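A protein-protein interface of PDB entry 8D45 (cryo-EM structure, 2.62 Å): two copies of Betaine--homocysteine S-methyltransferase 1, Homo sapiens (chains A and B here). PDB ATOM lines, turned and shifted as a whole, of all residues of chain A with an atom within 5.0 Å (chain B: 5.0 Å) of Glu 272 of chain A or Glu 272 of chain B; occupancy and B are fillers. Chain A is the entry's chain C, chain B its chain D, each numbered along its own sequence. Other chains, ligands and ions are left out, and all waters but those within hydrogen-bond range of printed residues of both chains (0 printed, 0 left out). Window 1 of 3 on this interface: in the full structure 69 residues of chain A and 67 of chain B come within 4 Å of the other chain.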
ATOM      1  N   PHE A 269       7.162   0.490  19.166  1.00  0.00           N
ATOM      2  CA  PHE A 269       7.744   1.561  18.374  1.00  0.00           C
ATOM      3  C   PHE A 269       8.817   1.084  17.405  1.00  0.00           C
ATOM      4  O   PHE A 269       9.763   1.832  17.137  1.00  0.00           O
ATOM      5  CB  PHE A 269       8.348   2.621  19.290  1.00  0.00           C
ATOM      6  CG  PHE A 269       7.422   3.101  20.355  1.00  0.00           C
ATOM      7  CD1 PHE A 269       6.157   3.558  20.041  1.00  0.00           C
ATOM      8  CD2 PHE A 269       7.823   3.118  21.675  1.00  0.00           C
ATOM      9  CE1 PHE A 269       5.307   4.000  21.027  1.00  0.00           C
ATOM     10  CE2 PHE A 269       6.980   3.568  22.662  1.00  0.00           C
ATOM     11  CZ  PHE A 269       5.723   4.011  22.336  1.00  0.00           C
ATOM     12  N   GLY A 270       8.706  -0.131  16.882  1.00  0.00           N
ATOM     13  CA  GLY A 270       9.680  -0.606  15.922  1.00  0.00           C
ATOM     14  C   GLY A 270       9.085  -1.466  14.832  1.00  0.00           C
ATOM     15  O   GLY A 270       9.812  -2.172  14.130  1.00  0.00           O
ATOM     16  N   LEU A 271       7.767  -1.414  14.669  1.00  0.00           N
ATOM     17  CA  LEU A 271       7.053  -2.334  13.797  1.00  0.00           C
ATOM     18  C   LEU A 271       6.822  -1.771  12.406  1.00  0.00           C
ATOM     19  O   LEU A 271       6.154  -2.418  11.596  1.00  0.00           O
ATOM     20  CB  LEU A 271       5.715  -2.721  14.425  1.00  0.00           C
ATOM     21  CG  LEU A 271       5.742  -3.102  15.906  1.00  0.00           C
ATOM     22  CD1 LEU A 271       4.350  -3.021  16.496  1.00  0.00           C
ATOM     23  CD2 LEU A 271       6.336  -4.487  16.088  1.00  0.00           C
ATOM     24  N   GLU A 272       7.353  -0.587  12.110  1.00  0.00           N
ATOM     25  CA  GLU A 272       7.161  -0.007  10.784  1.00  0.00           C
ATOM     26  C   GLU A 272       7.641  -0.924   9.667  1.00  0.00           C
ATOM     27  O   GLU A 272       6.938  -1.026   8.647  1.00  0.00           O
ATOM     28  CB  GLU A 272       7.868   1.352  10.710  1.00  0.00           C
ATOM     29  CG  GLU A 272       7.127   2.487  11.400  1.00  0.00           C
ATOM     30  CD  GLU A 272       7.374   2.525  12.898  1.00  0.00           C
ATOM     31  OE1 GLU A 272       8.202   1.735  13.388  1.00  0.00           O
ATOM     32  OE2 GLU A 272       6.754   3.355  13.589  1.00  0.00           O
ATOM     33  N   PRO A 273       8.799  -1.587   9.768  1.00  0.00           N
ATOM     34  CA  PRO A 273       9.191  -2.519   8.698  1.00  0.00           C
ATOM     35  C   PRO A 273       8.183  -3.627   8.466  1.00  0.00           C
ATOM     36  O   PRO A 273       7.921  -4.001   7.317  1.00  0.00           O
ATOM     37  CB  PRO A 273      10.525  -3.075   9.205  1.00  0.00           C
ATOM     38  CG  PRO A 273      11.042  -2.046  10.128  1.00  0.00           C
ATOM     39  CD  PRO A 273       9.843  -1.481  10.801  1.00  0.00           C
ATOM     40  N   ARG A 274       7.593  -4.151   9.541  1.00  0.00           N
ATOM     41  CA  ARG A 274       6.728  -5.319   9.449  1.00  0.00           C
ATOM     42  C   ARG A 274       5.387  -5.004   8.806  1.00  0.00           C
ATOM     43  O   ARG A 274       4.679  -5.932   8.408  1.00  0.00           O
ATOM     44  CB  ARG A 274       6.501  -5.896  10.842  1.00  0.00           C
ATOM     45  CG  ARG A 274       7.769  -6.265  11.586  1.00  0.00           C
ATOM     46  CD  ARG A 274       7.493  -6.382  13.066  1.00  0.00           C
ATOM     47  NE  ARG A 274       8.649  -6.836  13.827  1.00  0.00           N
ATOM     48  CZ  ARG A 274       9.112  -8.079  13.826  1.00  0.00           C
ATOM     49  NH1 ARG A 274       8.567  -9.022  13.078  1.00  0.00           N
ATOM     50  NH2 ARG A 274      10.149  -8.383  14.600  1.00  0.00           N
ATOM     51  N   VAL A 275       5.028  -3.722   8.691  1.00  0.00           N
ATOM     52  CA  VAL A 275       3.712  -3.342   8.191  1.00  0.00           C
ATOM     53  C   VAL A 275       3.477  -3.968   6.829  1.00  0.00           C
ATOM     54  O   VAL A 275       4.352  -3.954   5.959  1.00  0.00           O
ATOM     55  CB  VAL A 275       3.584  -1.810   8.129  1.00  0.00           C
ATOM     56  CG1 VAL A 275       2.331  -1.411   7.372  1.00  0.00           C
ATOM     57  CG2 VAL A 275       3.555  -1.222   9.520  1.00  0.00           C
ATOM     58  N   ALA A 276       2.281  -4.517   6.640  1.00  0.00           N
ATOM     59  CA  ALA A 276       1.904  -5.107   5.365  1.00  0.00           C
ATOM     60  C   ALA A 276       1.708  -4.029   4.312  1.00  0.00           C
ATOM     61  O   ALA A 276       1.551  -2.852   4.641  1.00  0.00           O
ATOM     62  CB  ALA A 276       0.622  -5.928   5.513  1.00  0.00           C
ATOM     63  N   THR A 277       1.717  -4.424   3.049  1.00  0.00           N
ATOM     64  CA  THR A 277       1.411  -3.544   1.937  1.00  0.00           C
ATOM     65  C   THR A 277      -0.038  -3.772   1.527  1.00  0.00           C
ATOM     66  O   THR A 277      -0.729  -4.632   2.068  1.00  0.00           O
ATOM     67  CB  THR A 277       2.363  -3.785   0.759  1.00  0.00           C
ATOM     68  OG1 THR A 277       1.989  -4.982   0.069  1.00  0.00           O
ATOM     69  CG2 THR A 277       3.799  -3.913   1.241  1.00  0.00           C
ATOM     70  N   ARG A 278      -0.501  -2.987   0.562  1.00  0.00           N
ATOM     71  CA  ARG A 278      -1.845  -3.181   0.043  1.00  0.00           C
ATOM     72  C   ARG A 278      -1.964  -4.445  -0.793  1.00  0.00           C
ATOM     73  O   ARG A 278      -3.077  -4.809  -1.180  1.00  0.00           O
ATOM     74  CB  ARG A 278      -2.266  -1.964  -0.776  1.00  0.00           C
ATOM     75  CG  ARG A 278      -1.487  -1.764  -2.058  1.00  0.00           C
ATOM     76  CD  ARG A 278      -1.707  -0.375  -2.619  1.00  0.00           C
ATOM     77  NE  ARG A 278      -1.319   0.653  -1.661  1.00  0.00           N
ATOM     78  CZ  ARG A 278      -1.768   1.899  -1.666  1.00  0.00           C
ATOM     79  NH1 ARG A 278      -2.656   2.311  -2.553  1.00  0.00           N
ATOM     80  NH2 ARG A 278      -1.319   2.753  -0.752  1.00  0.00           N
ATOM     81  N   TYR A 305      -6.158   2.460   3.871  1.00  0.00           N
ATOM     82  CA  TYR A 305      -5.792   1.885   2.581  1.00  0.00           C
ATOM     83  C   TYR A 305      -5.687   0.365   2.652  1.00  0.00           C
ATOM     84  O   TYR A 305      -5.929  -0.316   1.652  1.00  0.00           O
ATOM     85  CB  TYR A 305      -4.495   2.527   2.069  1.00  0.00           C
ATOM     86  CG  TYR A 305      -3.219   2.056   2.728  1.00  0.00           C
ATOM     87  CD1 TYR A 305      -2.826   2.561   3.955  1.00  0.00           C
ATOM     88  CD2 TYR A 305      -2.392   1.132   2.108  1.00  0.00           C
ATOM     89  CE1 TYR A 305      -1.671   2.142   4.558  1.00  0.00           C
ATOM     90  CE2 TYR A 305      -1.227   0.713   2.703  1.00  0.00           C
ATOM     91  CZ  TYR A 305      -0.873   1.221   3.929  1.00  0.00           C
ATOM     92  OH  TYR A 305       0.289   0.810   4.533  1.00  0.00           O
ATOM     93  N   PHE B 269       3.864   1.513  -4.340  1.00  0.00           N
ATOM     94  CA  PHE B 269       3.060   0.640  -3.494  1.00  0.00           C
ATOM     95  C   PHE B 269       3.857  -0.491  -2.862  1.00  0.00           C
ATOM     96  O   PHE B 269       3.311  -1.586  -2.676  1.00  0.00           O
ATOM     97  CB  PHE B 269       1.908   0.052  -4.301  1.00  0.00           C
ATOM     98  CG  PHE B 269       1.122   1.063  -5.066  1.00  0.00           C
ATOM     99  CD1 PHE B 269       0.604   2.177  -4.437  1.00  0.00           C
ATOM    100  CD2 PHE B 269       0.885   0.892  -6.416  1.00  0.00           C
ATOM    101  CE1 PHE B 269      -0.127   3.101  -5.143  1.00  0.00           C
ATOM    102  CE2 PHE B 269       0.156   1.814  -7.124  1.00  0.00           C
ATOM    103  CZ  PHE B 269      -0.351   2.918  -6.488  1.00  0.00           C
ATOM    104  N   GLY B 270       5.125  -0.275  -2.534  1.00  0.00           N
ATOM    105  CA  GLY B 270       5.903  -1.316  -1.897  1.00  0.00           C
ATOM    106  C   GLY B 270       6.879  -0.797  -0.868  1.00  0.00           C
ATOM    107  O   GLY B 270       7.799  -1.512  -0.467  1.00  0.00           O
ATOM    108  N   LEU B 271       6.689   0.440  -0.422  1.00  0.00           N
ATOM    109  CA  LEU B 271       7.670   1.130   0.399  1.00  0.00           C
ATOM    110  C   LEU B 271       7.370   1.041   1.886  1.00  0.00           C
ATOM    111  O   LEU B 271       8.079   1.661   2.682  1.00  0.00           O
ATOM    112  CB  LEU B 271       7.766   2.597  -0.020  1.00  0.00           C
ATOM    113  CG  LEU B 271       7.852   2.874  -1.521  1.00  0.00           C
ATOM    114  CD1 LEU B 271       7.482   4.313  -1.814  1.00  0.00           C
ATOM    115  CD2 LEU B 271       9.240   2.550  -2.046  1.00  0.00           C
ATOM    116  N   GLU B 272       6.342   0.291   2.280  1.00  0.00           N
ATOM    117  CA  GLU B 272       6.030   0.165   3.700  1.00  0.00           C
ATOM    118  C   GLU B 272       7.209  -0.347   4.518  1.00  0.00           C
ATOM    119  O   GLU B 272       7.437   0.184   5.618  1.00  0.00           O
ATOM    120  CB  GLU B 272       4.811  -0.746   3.891  1.00  0.00           C
ATOM    121  CG  GLU B 272       3.473  -0.111   3.535  1.00  0.00           C
ATOM    122  CD  GLU B 272       3.184  -0.129   2.044  1.00  0.00           C
ATOM    123  OE1 GLU B 272       3.861  -0.873   1.314  1.00  0.00           O
ATOM    124  OE2 GLU B 272       2.259   0.580   1.604  1.00  0.00           O
ATOM    125  N   PRO B 273       7.971  -1.355   4.076  1.00  0.00           N
ATOM    126  CA  PRO B 273       9.139  -1.774   4.868  1.00  0.00           C
ATOM    127  C   PRO B 273      10.144  -0.662   5.094  1.00  0.00           C
ATOM    128  O   PRO B 273      10.707  -0.543   6.188  1.00  0.00           O
ATOM    129  CB  PRO B 273       9.738  -2.904   4.024  1.00  0.00           C
ATOM    130  CG  PRO B 273       8.629  -3.394   3.186  1.00  0.00           C
ATOM    131  CD  PRO B 273       7.778  -2.210   2.893  1.00  0.00           C
ATOM    132  N   ARG B 274      10.368   0.173   4.079  1.00  0.00           N
ATOM    133  CA  ARG B 274      11.413   1.185   4.135  1.00  0.00           C
ATOM    134  C   ARG B 274      11.072   2.326   5.080  1.00  0.00           C
ATOM    135  O   ARG B 274      11.968   3.092   5.442  1.00  0.00           O
ATOM    136  CB  ARG B 274      11.661   1.738   2.736  1.00  0.00           C
ATOM    137  CG  ARG B 274      12.042   0.694   1.706  1.00  0.00           C
ATOM    138  CD  ARG B 274      11.821   1.229   0.310  1.00  0.00           C
ATOM    139  NE  ARG B 274      12.260   0.308  -0.729  1.00  0.00           N
ATOM    140  CZ  ARG B 274      13.527   0.058  -1.032  1.00  0.00           C
ATOM    141  NH1 ARG B 274      14.522   0.615  -0.364  1.00  0.00           N
ATOM    142  NH2 ARG B 274      13.801  -0.767  -2.036  1.00  0.00           N
ATOM    143  N   VAL B 275       9.806   2.452   5.488  1.00  0.00           N
ATOM    144  CA  VAL B 275       9.377   3.584   6.301  1.00  0.00           C
ATOM    145  C   VAL B 275      10.237   3.679   7.548  1.00  0.00           C
ATOM    146  O   VAL B 275      10.513   2.675   8.212  1.00  0.00           O
ATOM    147  CB  VAL B 275       7.886   3.452   6.663  1.00  0.00           C
ATOM    148  CG1 VAL B 275       7.498   4.500   7.688  1.00  0.00           C
ATOM    149  CG2 VAL B 275       7.022   3.595   5.432  1.00  0.00           C
ATOM    150  N   ALA B 276      10.656   4.896   7.873  1.00  0.00           N
ATOM    151  CA  ALA B 276      11.441   5.134   9.070  1.00  0.00           C
ATOM    152  C   ALA B 276      10.570   4.964  10.310  1.00  0.00           C
ATOM    153  O   ALA B 276       9.339   4.974  10.250  1.00  0.00           O
ATOM    154  CB  ALA B 276      12.052   6.531   9.032  1.00  0.00           C
ATOM    155  N   THR B 277      11.225   4.804  11.448  1.00  0.00           N
ATOM    156  CA  THR B 277      10.571   4.756  12.743  1.00  0.00           C
ATOM    157  C   THR B 277      10.677   6.134  13.382  1.00  0.00           C
ATOM    158  O   THR B 277      11.318   7.040  12.851  1.00  0.00           O
ATOM    159  CB  THR B 277      11.196   3.684  13.643  1.00  0.00           C
ATOM    160  OG1 THR B 277      12.526   4.068  14.003  1.00  0.00           O
ATOM    161  CG2 THR B 277      11.244   2.344  12.930  1.00  0.00           C
ATOM    162  N   ARG B 278      10.043   6.295  14.538  1.00  0.00           N
ATOM    163  CA  ARG B 278      10.167   7.544  15.271  1.00  0.00           C
ATOM    164  C   ARG B 278      11.550   7.723  15.875  1.00  0.00           C
ATOM    165  O   ARG B 278      11.845   8.799  16.402  1.00  0.00           O
ATOM    166  CB  ARG B 278       9.104   7.618  16.364  1.00  0.00           C
ATOM    167  CG  ARG B 278       9.257   6.588  17.464  1.00  0.00           C
ATOM    168  CD  ARG B 278       7.986   6.463  18.281  1.00  0.00           C
ATOM    169  NE  ARG B 278       6.848   6.095  17.448  1.00  0.00           N
ATOM    170  CZ  ARG B 278       5.582   6.347  17.743  1.00  0.00           C
ATOM    171  NH1 ARG B 278       5.243   6.989  18.848  1.00  0.00           N
ATOM    172  NH2 ARG B 278       4.630   5.948  16.907  1.00  0.00           N
ATOM    173  N   TYR B 305       3.397  11.520  13.423  1.00  0.00           N
ATOM    174  CA  TYR B 305       4.263  11.025  14.489  1.00  0.00           C
ATOM    175  C   TYR B 305       5.738  11.177  14.131  1.00  0.00           C
ATOM    176  O   TYR B 305       6.573  11.340  15.024  1.00  0.00           O
ATOM    177  CB  TYR B 305       3.897   9.574  14.828  1.00  0.00           C
ATOM    178  CG  TYR B 305       4.377   8.526  13.851  1.00  0.00           C
ATOM    179  CD1 TYR B 305       3.693   8.292  12.670  1.00  0.00           C
ATOM    180  CD2 TYR B 305       5.490   7.746  14.126  1.00  0.00           C
ATOM    181  CE1 TYR B 305       4.119   7.342  11.781  1.00  0.00           C
ATOM    182  CE2 TYR B 305       5.918   6.787  13.243  1.00  0.00           C
ATOM    183  CZ  TYR B 305       5.229   6.590  12.071  1.00  0.00           C
ATOM    184  OH  TYR B 305       5.645   5.633  11.181  1.00  0.00           O
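CZ of Arg 278 of chain B touches CD1 of Phe 269 of chain A (3.7 Å). Glu 272 of chain A touches Val 275 of chain B. Glu 272 of chain A touches Ala 276 of chain B. Glu 272 of chain A touches Thr 277 of chain B. Pro 273 of chain B touches Pro 273 of chain A. Val 275 of chain A touches Glu 272 of chain B (O to CB, 3.8 Å). Ala 276 of chain A touches Glu 272 of chain B. Glu 272 of chain B touches Thr 277 of chain A. CD1 of Phe 269 of chain B touches CZ of Arg 278 of chain A, 3.7 Å away. Glu 272 of chain B touches Tyr 305 of chain A (CG to OH, 3.5 Å).
Phe 269 of chain A touches Arg 278 of chain B, and with the chains exchanged Arg 278 of chain A touches Phe 269 of chain B. Glu 272 of chain A touches Val 275 of chain B, and with the chains exchanged Val 275 of chain A touches Glu 272 of chain B. Glu 272 of chain A touches Tyr 305 of chain B, and with the chains exchanged Tyr 305 of chain A touches Glu 272 of chain B. Pro 273 of chain B touches its own counterpart, Pro 273 of chain A.
The backbone carbonyl oxygen of Glu 272 of chain A lies close to the backbone carbonyl oxygen of Glu 272 of chain B, 3.3 Å away. OE2 of Glu 272 of chain A sits close to OH of Tyr 305 of chain B, at 3.5 Å.
Hydrophobic or aromatic side chains of chain A that line the printed part of chain B: Phe 269, Pro 273 and Tyr 305. Hydrophobic or aromatic side chains of chain B that line the printed part of chain A: Phe 269, Pro 273 and Tyr 305. Among the printed residues, 12 pairs touch across the chains. Among the printed residues, no Asp or Glu carboxylate lies within 4 Å of a Lys or Arg side-chain nitrogen of the other chain.
Glu 272 of chain A touches five residues of chain B. Of chain A, only Glu 272 (3.3 Å), Val 275 (3.8 Å), Ala 276 (3.5 Å), Thr 277 (3.0 Å) and Tyr 305 (3.5 Å) come within 4 Å of Glu 272 of chain B. Of the printed residues of chain B, Phe 269 of chain A touches Arg 278 (3.7 Å). Of the printed residues of chain A, Val 275 of chain B touches Glu 272. Of the printed residues of chain B, Thr 277 of chain A touches Glu 272. Printed residues of chain A within 4 Å of Phe 269 of chain B: Arg 278. Arg 274 of chain A touches none of the printed residues of chain B. Gly 270 of chain A touches none of the printed residues of chain B. The nearest residue of chain B that does not touch Glu 272 of chain A is Pro 273 of chain B (4.4 Å).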
